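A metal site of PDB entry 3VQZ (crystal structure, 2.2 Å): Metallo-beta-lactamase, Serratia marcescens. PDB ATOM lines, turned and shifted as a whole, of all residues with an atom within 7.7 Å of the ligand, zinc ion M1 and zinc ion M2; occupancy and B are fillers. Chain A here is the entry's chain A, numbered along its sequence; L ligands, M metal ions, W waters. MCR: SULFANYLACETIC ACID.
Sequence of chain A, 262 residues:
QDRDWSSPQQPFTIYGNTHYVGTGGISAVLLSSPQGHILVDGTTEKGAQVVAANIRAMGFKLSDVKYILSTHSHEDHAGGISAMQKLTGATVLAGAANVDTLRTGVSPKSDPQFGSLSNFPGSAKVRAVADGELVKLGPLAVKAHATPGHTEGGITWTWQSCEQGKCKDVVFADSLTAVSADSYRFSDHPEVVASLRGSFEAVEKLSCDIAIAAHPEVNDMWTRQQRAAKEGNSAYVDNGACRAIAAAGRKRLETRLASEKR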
ATOM      1  N   TRP A   5     -14.256  -8.054 -15.465  1.00  0.00           N
ATOM      2  CA  TRP A   5     -15.024  -7.091 -14.649  1.00  0.00           C
ATOM      3  C   TRP A   5     -14.194  -6.290 -13.683  1.00  0.00           C
ATOM      4  O   TRP A   5     -14.605  -5.185 -13.295  1.00  0.00           O
ATOM      5  CB  TRP A   5     -16.123  -7.800 -13.877  1.00  0.00           C
ATOM      6  CG  TRP A   5     -17.271  -8.347 -14.704  1.00  0.00           C
ATOM      7  CD1 TRP A   5     -17.561  -8.095 -16.046  1.00  0.00           C
ATOM      8  CD2 TRP A   5     -18.352  -9.228 -14.239  1.00  0.00           C
ATOM      9  NE1 TRP A   5     -18.706  -8.753 -16.433  1.00  0.00           N
ATOM     10  CE2 TRP A   5     -19.233  -9.452 -15.399  1.00  0.00           C
ATOM     11  CE3 TRP A   5     -18.667  -9.837 -13.034  1.00  0.00           C
ATOM     12  CZ2 TRP A   5     -20.360 -10.253 -15.317  1.00  0.00           C
ATOM     13  CZ3 TRP A   5     -19.816 -10.635 -12.960  1.00  0.00           C
ATOM     14  CH2 TRP A   5     -20.634 -10.835 -14.081  1.00  0.00           C
ATOM     15  N   GLY A  25     -14.044  -3.916 -17.868  1.00  0.00           N
ATOM     16  CA  GLY A  25     -15.323  -4.546 -18.191  1.00  0.00           C
ATOM     17  C   GLY A  25     -16.598  -3.913 -17.633  1.00  0.00           C
ATOM     18  O   GLY A  25     -17.683  -4.213 -18.111  1.00  0.00           O
ATOM     19  N   ILE A  26     -16.460  -3.048 -16.620  1.00  0.00           N
ATOM     20  CA  ILE A  26     -17.614  -2.366 -15.992  1.00  0.00           C
ATOM     21  C   ILE A  26     -17.397  -0.849 -15.944  1.00  0.00           C
ATOM     22  O   ILE A  26     -16.340  -0.368 -15.502  1.00  0.00           O
ATOM     23  CB  ILE A  26     -17.874  -2.887 -14.545  1.00  0.00           C
ATOM     24  CG1 ILE A  26     -18.047  -4.422 -14.516  1.00  0.00           C
ATOM     25  CG2 ILE A  26     -19.050  -2.182 -13.894  1.00  0.00           C
ATOM     26  CD1 ILE A  26     -19.319  -4.926 -15.181  1.00  0.00           C
ATOM     27  N   THR A  71     -26.693   2.392 -10.503  1.00  0.00           N
ATOM     28  CA  THR A  71     -27.622   2.018 -11.578  1.00  0.00           C
ATOM     29  C   THR A  71     -28.492   0.879 -11.064  1.00  0.00           C
ATOM     30  O   THR A  71     -29.700   1.066 -10.822  1.00  0.00           O
ATOM     31  CB  THR A  71     -26.882   1.615 -12.874  1.00  0.00           C
ATOM     32  OG1 THR A  71     -25.924   0.559 -12.619  1.00  0.00           O
ATOM     33  CG2 THR A  71     -26.186   2.828 -13.495  1.00  0.00           C
ATOM     34  N   HIS A  72     -27.877  -0.279 -10.856  1.00  0.00           N
ATOM     35  CA  HIS A  72     -28.571  -1.423 -10.265  1.00  0.00           C
ATOM     36  C   HIS A  72     -27.665  -2.233  -9.379  1.00  0.00           C
ATOM     37  O   HIS A  72     -26.436  -2.222  -9.522  1.00  0.00           O
ATOM     38  CB  HIS A  72     -29.273  -2.281 -11.325  1.00  0.00           C
ATOM     39  CG  HIS A  72     -28.346  -3.150 -12.146  1.00  0.00           C
ATOM     40  ND1 HIS A  72     -27.757  -2.727 -13.274  1.00  0.00           N
ATOM     41  CD2 HIS A  72     -27.961  -4.487 -11.986  1.00  0.00           C
ATOM     42  CE1 HIS A  72     -27.020  -3.731 -13.804  1.00  0.00           C
ATOM     43  NE2 HIS A  72     -27.138  -4.794 -13.020  1.00  0.00           N
ATOM     44  N   SER A  73     -28.277  -2.938  -8.439  1.00  0.00           N
ATOM     45  CA  SER A  73     -27.557  -3.611  -7.355  1.00  0.00           C
ATOM     46  C   SER A  73     -27.188  -5.062  -7.649  1.00  0.00           C
ATOM     47  O   SER A  73     -27.639  -5.968  -6.936  1.00  0.00           O
ATOM     48  CB  SER A  73     -28.382  -3.543  -6.070  1.00  0.00           C
ATOM     49  OG  SER A  73     -29.719  -3.947  -6.331  1.00  0.00           O
ATOM     50  N   HIS A  74     -26.396  -5.282  -8.696  1.00  0.00           N
ATOM     51  CA  HIS A  74     -25.716  -6.561  -8.923  1.00  0.00           C
ATOM     52  C   HIS A  74     -24.268  -6.387  -8.600  1.00  0.00           C
ATOM     53  O   HIS A  74     -23.750  -5.259  -8.659  1.00  0.00           O
ATOM     54  CB  HIS A  74     -25.877  -7.037 -10.362  1.00  0.00           C
ATOM     55  CG  HIS A  74     -27.257  -7.562 -10.682  1.00  0.00           C
ATOM     56  ND1 HIS A  74     -27.759  -7.572 -11.923  1.00  0.00           N
ATOM     57  CD2 HIS A  74     -28.247  -8.098  -9.854  1.00  0.00           C
ATOM     58  CE1 HIS A  74     -29.002  -8.091 -11.908  1.00  0.00           C
ATOM     59  NE2 HIS A  74     -29.303  -8.411 -10.632  1.00  0.00           N
ATOM     60  N   GLU A  75     -23.602  -7.497  -8.286  1.00  0.00           N
ATOM     61  CA  GLU A  75     -22.239  -7.477  -7.738  1.00  0.00           C
ATOM     62  C   GLU A  75     -21.207  -6.809  -8.641  1.00  0.00           C
ATOM     63  O   GLU A  75     -20.235  -6.250  -8.153  1.00  0.00           O
ATOM     64  CB  GLU A  75     -21.768  -8.910  -7.418  1.00  0.00           C
ATOM     65  CG  GLU A  75     -21.594  -9.786  -8.662  1.00  0.00           C
ATOM     66  CD  GLU A  75     -21.228 -11.242  -8.352  1.00  0.00           C
ATOM     67  OE1 GLU A  75     -20.509 -11.495  -7.359  1.00  0.00           O
ATOM     68  OE2 GLU A  75     -21.632 -12.131  -9.138  1.00  0.00           O
ATOM     69  N   ASP A  76     -21.438  -6.865  -9.946  1.00  0.00           N
ATOM     70  CA  ASP A  76     -20.468  -6.338 -10.889  1.00  0.00           C
ATOM     71  C   ASP A  76     -20.472  -4.805 -10.972  1.00  0.00           C
ATOM     72  O   ASP A  76     -19.474  -4.245 -11.370  1.00  0.00           O
ATOM     73  CB  ASP A  76     -20.595  -6.998 -12.283  1.00  0.00           C
ATOM     74  CG  ASP A  76     -21.983  -6.918 -12.869  1.00  0.00           C
ATOM     75  OD1 ASP A  76     -22.954  -6.903 -12.104  1.00  0.00           O
ATOM     76  OD2 ASP A  76     -22.102  -6.865 -14.104  1.00  0.00           O
ATOM     77  N   HIS A  77     -21.569  -4.142 -10.578  1.00  0.00           N
ATOM     78  CA  HIS A  77     -21.682  -2.664 -10.591  1.00  0.00           C
ATOM     79  C   HIS A  77     -21.648  -2.066  -9.227  1.00  0.00           C
ATOM     80  O   HIS A  77     -21.215  -0.924  -9.059  1.00  0.00           O
ATOM     81  CB  HIS A  77     -22.961  -2.187 -11.275  1.00  0.00           C
ATOM     82  CG  HIS A  77     -23.226  -2.908 -12.556  1.00  0.00           C
ATOM     83  ND1 HIS A  77     -22.734  -2.497 -13.734  1.00  0.00           N
ATOM     84  CD2 HIS A  77     -23.895  -4.105 -12.817  1.00  0.00           C
ATOM     85  CE1 HIS A  77     -23.081  -3.368 -14.705  1.00  0.00           C
ATOM     86  NE2 HIS A  77     -23.797  -4.357 -14.136  1.00  0.00           N
ATOM     87  N   ASP A 111     -35.428 -10.496  -7.715  1.00  0.00           N
ATOM     88  CA  ASP A 111     -34.270 -10.176  -8.578  1.00  0.00           C
ATOM     89  C   ASP A 111     -33.884 -11.369  -9.455  1.00  0.00           C
ATOM     90  O   ASP A 111     -33.643 -12.452  -8.950  1.00  0.00           O
ATOM     91  CB  ASP A 111     -33.091  -9.730  -7.690  1.00  0.00           C
ATOM     92  CG  ASP A 111     -31.781  -9.456  -8.459  1.00  0.00           C
ATOM     93  OD1 ASP A 111     -31.718  -9.499  -9.712  1.00  0.00           O
ATOM     94  OD2 ASP A 111     -30.765  -9.190  -7.794  1.00  0.00           O
ATOM     95  N   GLN A 113     -31.176 -12.175 -10.733  1.00  0.00           N
ATOM     96  CA  GLN A 113     -29.881 -12.742 -10.340  1.00  0.00           C
ATOM     97  C   GLN A 113     -29.774 -12.971  -8.840  1.00  0.00           C
ATOM     98  O   GLN A 113     -28.681 -13.089  -8.301  1.00  0.00           O
ATOM     99  CB  GLN A 113     -28.708 -11.899 -10.882  1.00  0.00           C
ATOM    100  CG  GLN A 113     -28.389 -12.223 -12.326  1.00  0.00           C
ATOM    101  CD  GLN A 113     -27.558 -11.157 -13.013  1.00  0.00           C
ATOM    102  OE1 GLN A 113     -26.595 -10.634 -12.429  1.00  0.00           O
ATOM    103  NE2 GLN A 113     -27.921 -10.823 -14.251  1.00  0.00           N
ATOM    104  N   HIS A 150     -34.440  -5.273 -15.225  1.00  0.00           N
ATOM    105  CA  HIS A 150     -33.228  -6.044 -15.004  1.00  0.00           C
ATOM    106  C   HIS A 150     -33.037  -6.185 -13.508  1.00  0.00           C
ATOM    107  O   HIS A 150     -32.627  -7.240 -13.037  1.00  0.00           O
ATOM    108  CB  HIS A 150     -32.023  -5.384 -15.677  1.00  0.00           C
ATOM    109  CG  HIS A 150     -30.718  -6.113 -15.456  1.00  0.00           C
ATOM    110  ND1 HIS A 150     -30.374  -7.223 -16.164  1.00  0.00           N
ATOM    111  CD2 HIS A 150     -29.674  -5.880 -14.557  1.00  0.00           C
ATOM    112  CE1 HIS A 150     -29.174  -7.667 -15.729  1.00  0.00           C
ATOM    113  NE2 HIS A 150     -28.742  -6.839 -14.768  1.00  0.00           N
ATOM    114  N   THR A 151     -33.355  -5.128 -12.772  1.00  0.00           N
ATOM    115  CA  THR A 151     -33.622  -5.181 -11.334  1.00  0.00           C
ATOM    116  C   THR A 151     -34.816  -4.265 -11.131  1.00  0.00           C
ATOM    117  O   THR A 151     -35.132  -3.461 -12.000  1.00  0.00           O
ATOM    118  CB  THR A 151     -32.475  -4.635 -10.455  1.00  0.00           C
ATOM    119  OG1 THR A 151     -32.336  -3.222 -10.689  1.00  0.00           O
ATOM    120  CG2 THR A 151     -31.168  -5.335 -10.743  1.00  0.00           C
ATOM    121  N   ASP A 174     -28.512   2.350 -17.422  1.00  0.00           N
ATOM    122  CA  ASP A 174     -28.629   1.075 -16.719  1.00  0.00           C
ATOM    123  C   ASP A 174     -28.920  -0.054 -17.723  1.00  0.00           C
ATOM    124  O   ASP A 174     -29.399   0.199 -18.858  1.00  0.00           O
ATOM    125  CB  ASP A 174     -29.725   1.189 -15.659  1.00  0.00           C
ATOM    126  CG  ASP A 174     -29.729   0.028 -14.683  1.00  0.00           C
ATOM    127  OD1 ASP A 174     -28.687  -0.642 -14.488  1.00  0.00           O
ATOM    128  OD2 ASP A 174     -30.802  -0.215 -14.106  1.00  0.00           O
ATOM    129  N   SER A 175     -28.630  -1.287 -17.314  1.00  0.00           N
ATOM    130  CA  SER A 175     -28.887  -2.480 -18.136  1.00  0.00           C
ATOM    131  C   SER A 175     -30.364  -2.751 -18.358  1.00  0.00           C
ATOM    132  O   SER A 175     -31.175  -2.668 -17.417  1.00  0.00           O
ATOM    133  CB  SER A 175     -28.261  -3.707 -17.505  1.00  0.00           C
ATOM    134  OG  SER A 175     -26.901  -3.466 -17.249  1.00  0.00           O
ATOM    135  N   LEU A 176     -30.698  -3.085 -19.592  1.00  0.00           N
ATOM    136  CA  LEU A 176     -32.068  -3.388 -19.986  1.00  0.00           C
ATOM    137  C   LEU A 176     -32.134  -4.847 -20.459  1.00  0.00           C
ATOM    138  O   LEU A 176     -32.928  -5.194 -21.342  1.00  0.00           O
ATOM    139  CB  LEU A 176     -32.507  -2.429 -21.111  1.00  0.00           C
ATOM    140  CG  LEU A 176     -32.400  -0.929 -20.828  1.00  0.00           C
ATOM    141  CD1 LEU A 176     -32.818  -0.124 -22.054  1.00  0.00           C
ATOM    142  CD2 LEU A 176     -33.248  -0.547 -19.602  1.00  0.00           C
ATOM    143  N   THR A 177     -31.292  -5.684 -19.865  1.00  0.00           N
ATOM    144  CA  THR A 177     -31.066  -7.049 -20.334  1.00  0.00           C
ATOM    145  C   THR A 177     -31.888  -8.097 -19.586  1.00  0.00           C
ATOM    146  O   THR A 177     -31.873  -8.169 -18.349  1.00  0.00           O
ATOM    147  CB  THR A 177     -29.574  -7.429 -20.207  1.00  0.00           C
ATOM    148  OG1 THR A 177     -29.133  -7.106 -18.873  1.00  0.00           O
ATOM    149  CG2 THR A 177     -28.733  -6.666 -21.236  1.00  0.00           C
ATOM    150  N   ALA A 178     -32.612  -8.900 -20.361  1.00  0.00           N
ATOM    151  CA  ALA A 178     -33.334 -10.044 -19.815  1.00  0.00           C
ATOM    152  C   ALA A 178     -32.342 -11.212 -19.656  1.00  0.00           C
ATOM    153  O   ALA A 178     -32.354 -12.153 -20.453  1.00  0.00           O
ATOM    154  CB  ALA A 178     -34.487 -10.440 -20.728  1.00  0.00           C
ATOM    155  N   VAL A 179     -31.466 -11.086 -18.662  1.00  0.00           N
ATOM    156  CA  VAL A 179     -30.546 -12.142 -18.255  1.00  0.00           C
ATOM    157  C   VAL A 179     -30.733 -12.372 -16.752  1.00  0.00           C
ATOM    158  O   VAL A 179     -31.165 -11.462 -16.035  1.00  0.00           O
ATOM    159  CB  VAL A 179     -29.048 -11.826 -18.574  1.00  0.00           C
ATOM    160  CG1 VAL A 179     -28.834 -11.653 -20.064  1.00  0.00           C
ATOM    161  CG2 VAL A 179     -28.528 -10.597 -17.822  1.00  0.00           C
ATOM    162  N   SER A 180     -30.415 -13.577 -16.291  1.00  0.00           N
ATOM    163  CA  SER A 180     -30.691 -13.971 -14.917  1.00  0.00           C
ATOM    164  C   SER A 180     -29.805 -15.135 -14.471  1.00  0.00           C
ATOM    165  O   SER A 180     -28.905 -15.550 -15.202  1.00  0.00           O
ATOM    166  CB  SER A 180     -32.142 -14.427 -14.827  1.00  0.00           C
ATOM    167  OG  SER A 180     -32.300 -15.587 -15.618  1.00  0.00           O
ATOM    168  N   ALA A 214     -23.775   0.727 -18.645  1.00  0.00           N
ATOM    169  CA  ALA A 214     -23.218   0.105 -17.444  1.00  0.00           C
ATOM    170  C   ALA A 214     -22.217  -0.999 -17.838  1.00  0.00           C
ATOM    171  O   ALA A 214     -21.130  -1.078 -17.258  1.00  0.00           O
ATOM    172  CB  ALA A 214     -24.320  -0.416 -16.534  1.00  0.00           C
ATOM    173  N   HIS A 215     -22.585  -1.820 -18.829  1.00  0.00           N
ATOM    174  CA  HIS A 215     -21.602  -2.658 -19.539  1.00  0.00           C
ATOM    175  C   HIS A 215     -21.097  -1.903 -20.754  1.00  0.00           C
ATOM    176  O   HIS A 215     -21.776  -1.853 -21.764  1.00  0.00           O
ATOM    177  CB  HIS A 215     -22.159  -4.041 -19.900  1.00  0.00           C
ATOM    178  CG  HIS A 215     -22.282  -4.970 -18.704  1.00  0.00           C
ATOM    179  ND1 HIS A 215     -21.326  -5.895 -18.393  1.00  0.00           N
ATOM    180  CD2 HIS A 215     -23.274  -5.085 -17.727  1.00  0.00           C
ATOM    181  CE1 HIS A 215     -21.698  -6.553 -17.264  1.00  0.00           C
ATOM    182  NE2 HIS A 215     -22.882  -6.049 -16.849  1.00  0.00           N
ATOM    183  N   GLU A 217     -19.246  -1.989 -23.384  1.00  0.00           N
ATOM    184  CA  GLU A 217     -19.292  -2.470 -24.790  1.00  0.00           C
ATOM    185  C   GLU A 217     -20.703  -2.430 -25.410  1.00  0.00           C
ATOM    186  O   GLU A 217     -20.857  -2.529 -26.632  1.00  0.00           O
ATOM    187  CB  GLU A 217     -18.654  -3.875 -24.916  1.00  0.00           C
ATOM    188  CG  GLU A 217     -19.486  -5.035 -24.360  1.00  0.00           C
ATOM    189  CD  GLU A 217     -19.531  -5.126 -22.836  1.00  0.00           C
ATOM    190  OE1 GLU A 217     -18.751  -4.459 -22.130  1.00  0.00           O
ATOM    191  OE2 GLU A 217     -20.355  -5.899 -22.313  1.00  0.00           O
ATOM    192  N   VAL A 218     -21.729  -2.266 -24.572  1.00  0.00           N
ATOM    193  CA  VAL A 218     -23.084  -2.178 -25.064  1.00  0.00           C
ATOM    194  C   VAL A 218     -23.270  -0.927 -25.956  1.00  0.00           C
ATOM    195  O   VAL A 218     -24.144  -0.899 -26.826  1.00  0.00           O
ATOM    196  CB  VAL A 218     -24.130  -2.252 -23.923  1.00  0.00           C
ATOM    197  CG1 VAL A 218     -25.537  -1.986 -24.437  1.00  0.00           C
ATOM    198  CG2 VAL A 218     -24.059  -3.628 -23.244  1.00  0.00           C
ATOM    199  N   ARG A 252     -33.409  -8.883 -27.416  1.00  0.00           N
ATOM    200  CA  ARG A 252     -32.927  -9.857 -26.439  1.00  0.00           C
ATOM    201  C   ARG A 252     -34.043 -10.481 -25.578  1.00  0.00           C
ATOM    202  O   ARG A 252     -34.043 -11.678 -25.334  1.00  0.00           O
ATOM    203  CB  ARG A 252     -31.813  -9.261 -25.573  1.00  0.00           C
ATOM    204  CG  ARG A 252     -31.263 -10.238 -24.544  1.00  0.00           C
ATOM    205  CD  ARG A 252     -30.427  -9.538 -23.489  1.00  0.00           C
ATOM    206  NE  ARG A 252     -29.045  -9.297 -23.916  1.00  0.00           N
ATOM    207  CZ  ARG A 252     -28.152 -10.247 -24.173  1.00  0.00           C
ATOM    208  NH1 ARG A 252     -28.491 -11.535 -24.087  1.00  0.00           N
ATOM    209  NH2 ARG A 252     -26.919  -9.923 -24.519  1.00  0.00           N
HETATM  210  OXT MCR L   1     -26.567  -6.753 -18.159  1.00  0.00           O
HETATM  211  C   MCR L   1     -26.115  -6.744 -16.985  1.00  0.00           C
HETATM  212  O   MCR L   1     -25.997  -5.684 -16.323  1.00  0.00           O
HETATM  213  CA  MCR L   1     -25.693  -8.059 -16.366  1.00  0.00           C
HETATM  214  S2  MCR L   1     -25.371  -7.867 -14.590  1.00  0.00           S
HETATM  215 ZN    ZN M   1     -23.777  -6.149 -15.053  1.00  0.00          ZN
HETATM  216 ZN    ZN M   2     -27.017  -6.805 -13.637  1.00  0.00          ZN
HETATM  217  O   HOH W   1     -26.153  -4.739 -20.353  1.00  0.00           O
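OG of Ser 175 lies close to OXT of the ligand, 3.4 Å away. OG1 of Thr 177 is in hydrogen-bond range of OXT of the ligand (2.7 Å). S2 of the ligand lies close to OE1 of Gln 113, at 3.7 Å.
ND1 of His 150 sits at hydrogen-bond distance from O of Thr 177, 2.8 Å away. ND1 of His 72 lies within hydrogen-bond range of OD1 of Asp 174, at 2.6 Å. ND1 of His 74 lies close to OE1 of Gln 113 (3.3 Å). NE2 of His 74 sits at hydrogen-bond distance from OD1 of Asp 111, 2.8 Å away. The backbone NH (N) of Gln 113 sits at hydrogen-bond distance from the side-chain carboxylate (OD1) of Asp 111.
Hydrophobic or aromatic side chains within 4 Å of the ligand: His 72, His 150 and His 215. Within 4 Å of the ligand: His 72, His 74, Asp 76, His 77, Gln 113, His 150, Ser 175, Thr 177 and His 215. The nearest printed residue that does not touch the ligand is Val 179 (4.1 Å).
Three residues have an atom within 4 Å of zinc ion M1: Asp 76, His 77 and His 215. The nearest printed residue that does not touch zinc ion M1 is His 72 (4.2 Å).
The nearest printed residue that does not touch zinc ion M2 is Gln 113 (4.04 Å).
Zinc ion M1 is bound by NE2 of His 215, NE2 of His 77, OD2 of Asp 76, S2 of the ligand and O of the ligand. Zinc ion M1 has five donor atoms within binding distance.
Zinc ion M2 is bound by a ring nitrogen (ND1) of His 74 (2.0 Å), a ring nitrogen (NE2) of His 150 (2.1 Å), a ring nitrogen (NE2) of His 72 (2.1 Å) and a sulfur (S2) of the ligand (2.2 Å). Zinc ion M2 has four donor atoms within binding distance.
Water W1 lies within hydrogen-bond range of OXT of the ligand and OG of Ser 175.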
